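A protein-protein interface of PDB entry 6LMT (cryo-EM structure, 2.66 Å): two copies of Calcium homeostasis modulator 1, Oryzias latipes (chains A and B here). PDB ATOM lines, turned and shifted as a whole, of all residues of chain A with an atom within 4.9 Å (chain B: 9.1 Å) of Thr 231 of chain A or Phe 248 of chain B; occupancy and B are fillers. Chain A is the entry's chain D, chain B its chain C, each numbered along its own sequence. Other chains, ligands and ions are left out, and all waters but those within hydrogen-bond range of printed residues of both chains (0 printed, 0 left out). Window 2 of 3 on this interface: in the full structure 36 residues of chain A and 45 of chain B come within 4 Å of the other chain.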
ATOM      1  N   MET A 227     -16.214   9.937  23.053  1.00  0.00           N
ATOM      2  CA  MET A 227     -17.343   9.120  22.625  1.00  0.00           C
ATOM      3  C   MET A 227     -18.663   9.653  23.154  1.00  0.00           C
ATOM      4  O   MET A 227     -19.698   9.474  22.505  1.00  0.00           O
ATOM      5  CB  MET A 227     -17.163   7.664  23.055  1.00  0.00           C
ATOM      6  CG  MET A 227     -16.055   6.944  22.326  1.00  0.00           C
ATOM      7  SD  MET A 227     -16.004   5.209  22.770  1.00  0.00           S
ATOM      8  CE  MET A 227     -17.417   4.603  21.863  1.00  0.00           C
ATOM      9  N   PHE A 228     -18.648  10.332  24.301  1.00  0.00           N
ATOM     10  CA  PHE A 228     -19.853  11.010  24.755  1.00  0.00           C
ATOM     11  C   PHE A 228     -20.183  12.215  23.881  1.00  0.00           C
ATOM     12  O   PHE A 228     -21.366  12.514  23.679  1.00  0.00           O
ATOM     13  CB  PHE A 228     -19.701  11.432  26.213  1.00  0.00           C
ATOM     14  CG  PHE A 228     -20.935  12.037  26.795  1.00  0.00           C
ATOM     15  CD1 PHE A 228     -22.018  11.244  27.119  1.00  0.00           C
ATOM     16  CD2 PHE A 228     -21.017  13.398  27.018  1.00  0.00           C
ATOM     17  CE1 PHE A 228     -23.162  11.793  27.652  1.00  0.00           C
ATOM     18  CE2 PHE A 228     -22.163  13.950  27.552  1.00  0.00           C
ATOM     19  CZ  PHE A 228     -23.235  13.144  27.869  1.00  0.00           C
ATOM     20  N   ASP A 229     -19.170  12.896  23.333  1.00  0.00           N
ATOM     21  CA  ASP A 229     -19.434  14.047  22.468  1.00  0.00           C
ATOM     22  C   ASP A 229     -20.082  13.629  21.159  1.00  0.00           C
ATOM     23  O   ASP A 229     -21.093  14.210  20.751  1.00  0.00           O
ATOM     24  CB  ASP A 229     -18.154  14.829  22.185  1.00  0.00           C
ATOM     25  CG  ASP A 229     -17.722  15.681  23.347  1.00  0.00           C
ATOM     26  OD1 ASP A 229     -18.592  16.114  24.124  1.00  0.00           O
ATOM     27  OD2 ASP A 229     -16.508  15.928  23.480  1.00  0.00           O
ATOM     28  N   GLU A 230     -19.522  12.624  20.480  1.00  0.00           N
ATOM     29  CA  GLU A 230     -20.135  12.199  19.228  1.00  0.00           C
ATOM     30  C   GLU A 230     -21.438  11.447  19.427  1.00  0.00           C
ATOM     31  O   GLU A 230     -22.237  11.378  18.488  1.00  0.00           O
ATOM     32  CB  GLU A 230     -19.197  11.340  18.381  1.00  0.00           C
ATOM     33  CG  GLU A 230     -18.178  12.125  17.559  1.00  0.00           C
ATOM     34  CD  GLU A 230     -16.782  12.125  18.132  1.00  0.00           C
ATOM     35  OE1 GLU A 230     -16.532  11.360  19.078  1.00  0.00           O
ATOM     36  OE2 GLU A 230     -15.921  12.869  17.616  1.00  0.00           O
ATOM     37  N   THR A 231     -21.688  10.889  20.610  1.00  0.00           N
ATOM     38  CA  THR A 231     -22.978  10.244  20.815  1.00  0.00           C
ATOM     39  C   THR A 231     -24.066  11.283  21.040  1.00  0.00           C
ATOM     40  O   THR A 231     -25.197  11.116  20.568  1.00  0.00           O
ATOM     41  CB  THR A 231     -22.906   9.259  21.979  1.00  0.00           C
ATOM     42  OG1 THR A 231     -21.831   8.344  21.748  1.00  0.00           O
ATOM     43  CG2 THR A 231     -24.185   8.455  22.085  1.00  0.00           C
ATOM     44  N   CYS A 232     -23.733  12.378  21.733  1.00  0.00           N
ATOM     45  CA  CYS A 232     -24.673  13.491  21.846  1.00  0.00           C
ATOM     46  C   CYS A 232     -24.973  14.102  20.486  1.00  0.00           C
ATOM     47  O   CYS A 232     -26.115  14.486  20.218  1.00  0.00           O
ATOM     48  CB  CYS A 232     -24.139  14.563  22.794  1.00  0.00           C
ATOM     49  SG  CYS A 232     -24.152  14.143  24.541  1.00  0.00           S
ATOM     50  N   LYS A 233     -23.975  14.163  19.599  1.00  0.00           N
ATOM     51  CA  LYS A 233     -24.205  14.749  18.281  1.00  0.00           C
ATOM     52  C   LYS A 233     -25.083  13.868  17.404  1.00  0.00           C
ATOM     53  O   LYS A 233     -25.890  14.387  16.631  1.00  0.00           O
ATOM     54  CB  LYS A 233     -22.881  15.030  17.582  1.00  0.00           C
ATOM     55  CG  LYS A 233     -22.084  16.122  18.237  1.00  0.00           C
ATOM     56  CD  LYS A 233     -20.760  16.333  17.547  1.00  0.00           C
ATOM     57  CE  LYS A 233     -19.935  17.365  18.291  1.00  0.00           C
ATOM     58  NZ  LYS A 233     -18.610  17.588  17.664  1.00  0.00           N
ATOM     59  N   GLU A 234     -24.959  12.547  17.502  1.00  0.00           N
ATOM     60  CA  GLU A 234     -25.824  11.714  16.678  1.00  0.00           C
ATOM     61  C   GLU A 234     -27.238  11.616  17.246  1.00  0.00           C
ATOM     62  O   GLU A 234     -28.199  11.488  16.477  1.00  0.00           O
ATOM     63  CB  GLU A 234     -25.201  10.328  16.484  1.00  0.00           C
ATOM     64  CG  GLU A 234     -25.068   9.473  17.721  1.00  0.00           C
ATOM     65  CD  GLU A 234     -24.442   8.132  17.416  1.00  0.00           C
ATOM     66  OE1 GLU A 234     -24.056   7.915  16.249  1.00  0.00           O
ATOM     67  OE2 GLU A 234     -24.353   7.289  18.335  1.00  0.00           O
ATOM     68  N   HIS A 235     -27.400  11.705  18.567  1.00  0.00           N
ATOM     69  CA  HIS A 235     -28.738  11.825  19.131  1.00  0.00           C
ATOM     70  C   HIS A 235     -29.339  13.202  18.911  1.00  0.00           C
ATOM     71  O   HIS A 235     -30.564  13.345  18.971  1.00  0.00           O
ATOM     72  CB  HIS A 235     -28.732  11.497  20.623  1.00  0.00           C
ATOM     73  CG  HIS A 235     -28.631  10.036  20.917  1.00  0.00           C
ATOM     74  ND1 HIS A 235     -29.709   9.184  20.814  1.00  0.00           N
ATOM     75  CD2 HIS A 235     -27.580   9.268  21.286  1.00  0.00           C
ATOM     76  CE1 HIS A 235     -29.329   7.957  21.120  1.00  0.00           C
ATOM     77  NE2 HIS A 235     -28.040   7.980  21.406  1.00  0.00           N
ATOM     78  N   ALA B 240     -16.044   1.995  27.080  1.00  0.00           N
ATOM     79  CA  ALA B 240     -16.645   3.320  26.990  1.00  0.00           C
ATOM     80  C   ALA B 240     -17.910   3.291  26.147  1.00  0.00           C
ATOM     81  O   ALA B 240     -18.869   4.004  26.449  1.00  0.00           O
ATOM     82  CB  ALA B 240     -15.644   4.329  26.429  1.00  0.00           C
ATOM     83  N   LYS B 241     -17.937   2.468  25.094  1.00  0.00           N
ATOM     84  CA  LYS B 241     -19.162   2.286  24.321  1.00  0.00           C
ATOM     85  C   LYS B 241     -20.272   1.667  25.163  1.00  0.00           C
ATOM     86  O   LYS B 241     -21.445   2.022  24.994  1.00  0.00           O
ATOM     87  CB  LYS B 241     -18.874   1.425  23.093  1.00  0.00           C
ATOM     88  CG  LYS B 241     -20.062   1.169  22.182  1.00  0.00           C
ATOM     89  CD  LYS B 241     -19.637   0.413  20.937  1.00  0.00           C
ATOM     90  CE  LYS B 241     -19.280  -1.031  21.268  1.00  0.00           C
ATOM     91  NZ  LYS B 241     -18.988  -1.842  20.043  1.00  0.00           N
ATOM     92  N   VAL B 242     -19.913   0.781  26.095  1.00  0.00           N
ATOM     93  CA  VAL B 242     -20.905   0.182  26.984  1.00  0.00           C
ATOM     94  C   VAL B 242     -21.512   1.239  27.900  1.00  0.00           C
ATOM     95  O   VAL B 242     -22.737   1.309  28.066  1.00  0.00           O
ATOM     96  CB  VAL B 242     -20.273  -0.968  27.790  1.00  0.00           C
ATOM     97  CG1 VAL B 242     -21.256  -1.517  28.810  1.00  0.00           C
ATOM     98  CG2 VAL B 242     -19.830  -2.074  26.866  1.00  0.00           C
ATOM     99  N   CYS B 243     -20.670   2.107  28.467  1.00  0.00           N
ATOM    100  CA  CYS B 243     -21.151   3.074  29.452  1.00  0.00           C
ATOM    101  C   CYS B 243     -21.970   4.183  28.807  1.00  0.00           C
ATOM    102  O   CYS B 243     -22.973   4.626  29.379  1.00  0.00           O
ATOM    103  CB  CYS B 243     -19.974   3.663  30.222  1.00  0.00           C
ATOM    104  SG  CYS B 243     -19.127   2.477  31.278  1.00  0.00           S
ATOM    105  N   ILE B 244     -21.575   4.633  27.616  1.00  0.00           N
ATOM    106  CA  ILE B 244     -22.280   5.732  26.960  1.00  0.00           C
ATOM    107  C   ILE B 244     -23.656   5.282  26.484  1.00  0.00           C
ATOM    108  O   ILE B 244     -24.657   5.992  26.663  1.00  0.00           O
ATOM    109  CB  ILE B 244     -21.430   6.299  25.810  1.00  0.00           C
ATOM    110  CG1 ILE B 244     -20.155   6.950  26.357  1.00  0.00           C
ATOM    111  CG2 ILE B 244     -22.207   7.272  24.989  1.00  0.00           C
ATOM    112  CD1 ILE B 244     -20.407   7.995  27.389  1.00  0.00           C
ATOM    113  N   HIS B 245     -23.733   4.079  25.903  1.00  0.00           N
ATOM    114  CA  HIS B 245     -25.008   3.565  25.411  1.00  0.00           C
ATOM    115  C   HIS B 245     -25.975   3.296  26.557  1.00  0.00           C
ATOM    116  O   HIS B 245     -27.171   3.588  26.444  1.00  0.00           O
ATOM    117  CB  HIS B 245     -24.779   2.294  24.595  1.00  0.00           C
ATOM    118  CG  HIS B 245     -25.988   1.829  23.846  1.00  0.00           C
ATOM    119  ND1 HIS B 245     -26.080   0.571  23.295  1.00  0.00           N
ATOM    120  CD2 HIS B 245     -27.145   2.460  23.537  1.00  0.00           C
ATOM    121  CE1 HIS B 245     -27.246   0.442  22.687  1.00  0.00           C
ATOM    122  NE2 HIS B 245     -27.912   1.574  22.822  1.00  0.00           N
ATOM    123  N   GLN B 246     -25.467   2.783  27.679  1.00  0.00           N
ATOM    124  CA  GLN B 246     -26.300   2.566  28.852  1.00  0.00           C
ATOM    125  C   GLN B 246     -26.737   3.876  29.504  1.00  0.00           C
ATOM    126  O   GLN B 246     -27.803   3.916  30.131  1.00  0.00           O
ATOM    127  CB  GLN B 246     -25.550   1.671  29.847  1.00  0.00           C
ATOM    128  CG  GLN B 246     -26.360   1.206  31.044  1.00  0.00           C
ATOM    129  CD  GLN B 246     -27.537   0.336  30.645  1.00  0.00           C
ATOM    130  OE1 GLN B 246     -27.417  -0.536  29.787  1.00  0.00           O
ATOM    131  NE2 GLN B 246     -28.688   0.581  31.259  1.00  0.00           N
ATOM    132  N   TYR B 247     -25.963   4.953  29.344  1.00  0.00           N
ATOM    133  CA  TYR B 247     -26.398   6.251  29.856  1.00  0.00           C
ATOM    134  C   TYR B 247     -27.596   6.787  29.078  1.00  0.00           C
ATOM    135  O   TYR B 247     -28.569   7.266  29.673  1.00  0.00           O
ATOM    136  CB  TYR B 247     -25.250   7.262  29.804  1.00  0.00           C
ATOM    137  CG  TYR B 247     -25.658   8.608  30.336  1.00  0.00           C
ATOM    138  CD1 TYR B 247     -25.798   8.811  31.701  1.00  0.00           C
ATOM    139  CD2 TYR B 247     -25.927   9.669  29.480  1.00  0.00           C
ATOM    140  CE1 TYR B 247     -26.191  10.030  32.204  1.00  0.00           C
ATOM    141  CE2 TYR B 247     -26.323  10.895  29.973  1.00  0.00           C
ATOM    142  CZ  TYR B 247     -26.444  11.070  31.338  1.00  0.00           C
ATOM    143  OH  TYR B 247     -26.845  12.277  31.845  1.00  0.00           O
ATOM    144  N   PHE B 248     -27.546   6.717  27.753  1.00  0.00           N
ATOM    145  CA  PHE B 248     -28.643   7.226  26.944  1.00  0.00           C
ATOM    146  C   PHE B 248     -29.853   6.303  26.904  1.00  0.00           C
ATOM    147  O   PHE B 248     -30.865   6.691  26.320  1.00  0.00           O
ATOM    148  CB  PHE B 248     -28.170   7.514  25.523  1.00  0.00           C
ATOM    149  CG  PHE B 248     -27.354   8.761  25.404  1.00  0.00           C
ATOM    150  CD1 PHE B 248     -27.972   9.996  25.348  1.00  0.00           C
ATOM    151  CD2 PHE B 248     -25.975   8.705  25.350  1.00  0.00           C
ATOM    152  CE1 PHE B 248     -27.229  11.155  25.239  1.00  0.00           C
ATOM    153  CE2 PHE B 248     -25.226   9.866  25.243  1.00  0.00           C
ATOM    154  CZ  PHE B 248     -25.856  11.088  25.185  1.00  0.00           C
ATOM    155  N   GLU B 249     -29.787   5.110  27.502  1.00  0.00           N
ATOM    156  CA  GLU B 249     -30.992   4.295  27.653  1.00  0.00           C
ATOM    157  C   GLU B 249     -32.005   4.975  28.562  1.00  0.00           C
ATOM    158  O   GLU B 249     -33.218   4.868  28.349  1.00  0.00           O
ATOM    159  CB  GLU B 249     -30.647   2.913  28.207  1.00  0.00           C
ATOM    160  CG  GLU B 249     -29.857   2.034  27.266  1.00  0.00           C
ATOM    161  CD  GLU B 249     -30.622   1.681  26.008  1.00  0.00           C
ATOM    162  OE1 GLU B 249     -31.859   1.513  26.081  1.00  0.00           O
ATOM    163  OE2 GLU B 249     -29.982   1.583  24.940  1.00  0.00           O
ATOM    164  N   ASN B 250     -31.523   5.677  29.583  1.00  0.00           N
ATOM    165  CA  ASN B 250     -32.423   6.302  30.542  1.00  0.00           C
ATOM    166  C   ASN B 250     -32.658   7.768  30.203  1.00  0.00           C
ATOM    167  O   ASN B 250     -33.780   8.278  30.340  1.00  0.00           O
ATOM    168  CB  ASN B 250     -31.839   6.152  31.944  1.00  0.00           C
ATOM    169  CG  ASN B 250     -31.612   4.699  32.317  1.00  0.00           C
ATOM    170  OD1 ASN B 250     -30.475   4.264  32.496  1.00  0.00           O
ATOM    171  ND2 ASN B 250     -32.693   3.935  32.418  1.00  0.00           N
ATOM    172  N   ILE B 251     -31.619   8.458  29.738  1.00  0.00           N
ATOM    173  CA  ILE B 251     -31.737   9.897  29.556  1.00  0.00           C
ATOM    174  C   ILE B 251     -32.500  10.233  28.280  1.00  0.00           C
ATOM    175  O   ILE B 251     -33.228  11.230  28.245  1.00  0.00           O
ATOM    176  CB  ILE B 251     -30.335  10.521  29.618  1.00  0.00           C
ATOM    177  CG1 ILE B 251     -29.719  10.159  30.964  1.00  0.00           C
ATOM    178  CG2 ILE B 251     -30.367  12.031  29.469  1.00  0.00           C
ATOM    179  CD1 ILE B 251     -30.494  10.669  32.157  1.00  0.00           C
ATOM    180  N   SER B 252     -32.416   9.391  27.240  1.00  0.00           N
ATOM    181  CA  SER B 252     -33.300   9.580  26.091  1.00  0.00           C
ATOM    182  C   SER B 252     -34.753   9.278  26.426  1.00  0.00           C
ATOM    183  O   SER B 252     -35.644   9.761  25.721  1.00  0.00           O
ATOM    184  CB  SER B 252     -32.867   8.717  24.909  1.00  0.00           C
ATOM    185  OG  SER B 252     -33.003   7.344  25.223  1.00  0.00           O
ATOM    186  N   GLY B 253     -35.011   8.505  27.484  1.00  0.00           N
ATOM    187  CA  GLY B 253     -36.364   8.419  28.009  1.00  0.00           C
ATOM    188  C   GLY B 253     -36.845   9.743  28.571  1.00  0.00           C
ATOM    189  O   GLY B 253     -38.042  10.041  28.554  1.00  0.00           O
ATOM    190  N   GLU B 254     -35.916  10.553  29.084  1.00  0.00           N
ATOM    191  CA  GLU B 254     -36.250  11.922  29.470  1.00  0.00           C
ATOM    192  C   GLU B 254     -36.195  12.882  28.287  1.00  0.00           C
ATOM    193  O   GLU B 254     -37.016  13.803  28.203  1.00  0.00           O
ATOM    194  CB  GLU B 254     -35.317  12.389  30.583  1.00  0.00           C
ATOM    195  CG  GLU B 254     -35.633  11.781  31.930  1.00  0.00           C
ATOM    196  CD  GLU B 254     -34.604  12.129  32.978  1.00  0.00           C
ATOM    197  OE1 GLU B 254     -33.527  12.626  32.598  1.00  0.00           O
ATOM    198  OE2 GLU B 254     -34.878  11.925  34.181  1.00  0.00           O
ATOM    199  N   MET B 255     -35.272  12.671  27.342  1.00  0.00           N
ATOM    200  CA  MET B 255     -35.151  13.524  26.160  1.00  0.00           C
ATOM    201  C   MET B 255     -36.321  13.382  25.188  1.00  0.00           C
ATOM    202  O   MET B 255     -36.389  14.154  24.224  1.00  0.00           O
ATOM    203  CB  MET B 255     -33.846  13.241  25.405  1.00  0.00           C
ATOM    204  CG  MET B 255     -32.545  13.583  26.135  1.00  0.00           C
ATOM    205  SD  MET B 255     -32.331  15.301  26.632  1.00  0.00           S
ATOM    206  CE  MET B 255     -32.566  15.199  28.401  1.00  0.00           C
ATOM    207  N   GLN B 256     -37.207  12.403  25.399  1.00  0.00           N
ATOM    208  CA  GLN B 256     -38.503  12.373  24.729  1.00  0.00           C
ATOM    209  C   GLN B 256     -39.270  13.672  24.957  1.00  0.00           C
ATOM    210  O   GLN B 256     -39.493  14.453  24.027  1.00  0.00           O
ATOM    211  CB  GLN B 256     -39.317  11.186  25.244  1.00  0.00           C
ATOM    212  CG  GLN B 256     -38.773   9.831  24.853  1.00  0.00           C
ATOM    213  CD  GLN B 256     -39.488   8.694  25.550  1.00  0.00           C
ATOM    214  OE1 GLN B 256     -40.369   8.913  26.380  1.00  0.00           O
ATOM    215  NE2 GLN B 256     -39.097   7.470  25.231  1.00  0.00           N
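No position is printed for both chains. Of the 8 pairs that touch across the chains among the printed residues, none has its exchanged pair printed and touching as well.
Among the printed residues, merely in contact across the chains: Thr 231 of chain A with Ile 244 of chain B (3.4 Å), Cys 232 of chain A with Phe 248 of chain B (3.6 Å), Thr 231 of chain A with Phe 248 of chain B (3.6 Å), Phe 228 of chain A with Ile 244 of chain B (3.6 Å), Met 227 of chain A with Lys 241 of chain B (3.7 Å), Phe 228 of chain A with Phe 248 of chain B (3.7 Å), Met 227 of chain A with Ala 240 of chain B (3.8 Å) and Phe 228 of chain A with Tyr 247 of chain B (3.9 Å).
OG of Ser 252 of chain B sits at hydrogen-bond distance from O of Phe 248 of chain B (2.5 Å). The side-chain hydroxyl (OG1) of Thr 231 of chain A is in hydrogen-bond range of the backbone carbonyl oxygen (O) of Met 227 of chain A (2.5 Å). SG of Cys 232 of chain A lies within hydrogen-bond range of O of Phe 228 of chain A (3.3 Å).
Of the printed residues of chain B, Met 227 of chain A touches Ala 240 (3.8 Å) and Lys 241 (3.7 Å). Printed residues of chain B within 4 Å of Phe 228 of chain A: Ile 244, Tyr 247 and Phe 248. Thr 231 of chain A touches just these residues of chain B: Ile 244 (3.4 Å) and Phe 248 (3.6 Å). Of chain B, only Phe 248 (3.6 Å) comes within 4 Å of Cys 232 of chain A. Printed residues of chain A within 4 Å of Lys 241 of chain B: Met 227 (3.7 Å). Of the printed residues of chain A, Ile 244 of chain B touches Phe 228 (3.6 Å) and Thr 231 (3.4 Å). Printed residues of chain A within 4 Å of Tyr 247 of chain B: Phe 228 (3.9 Å). Of chain A, only Phe 228, Thr 231 and Cys 232 come within 4 Å of Phe 248 of chain B. The nearest residue of chain A that does not touch Phe 248 of chain B is His 235 of chain A (4.1 Å). The nearest printed residue of chain A that does not touch Ile 244 of chain B is Met 227 of chain A (4.2 Å).
Of the 9 printed residues of chain A, 4 touch a printed residue of chain B. Along chain A the printed residues that touch a printed residue of chain B span positions 227 to 232. Printed residues of chain B that touch a printed residue of chain A: Ala 240, Lys 241, Ile 244, Tyr 247 and Phe 248. Hydrophobic or aromatic side chains of chain B within 4 Å of the printed part of chain A: Ala 240, Ile 244, Tyr 247 and Phe 248.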
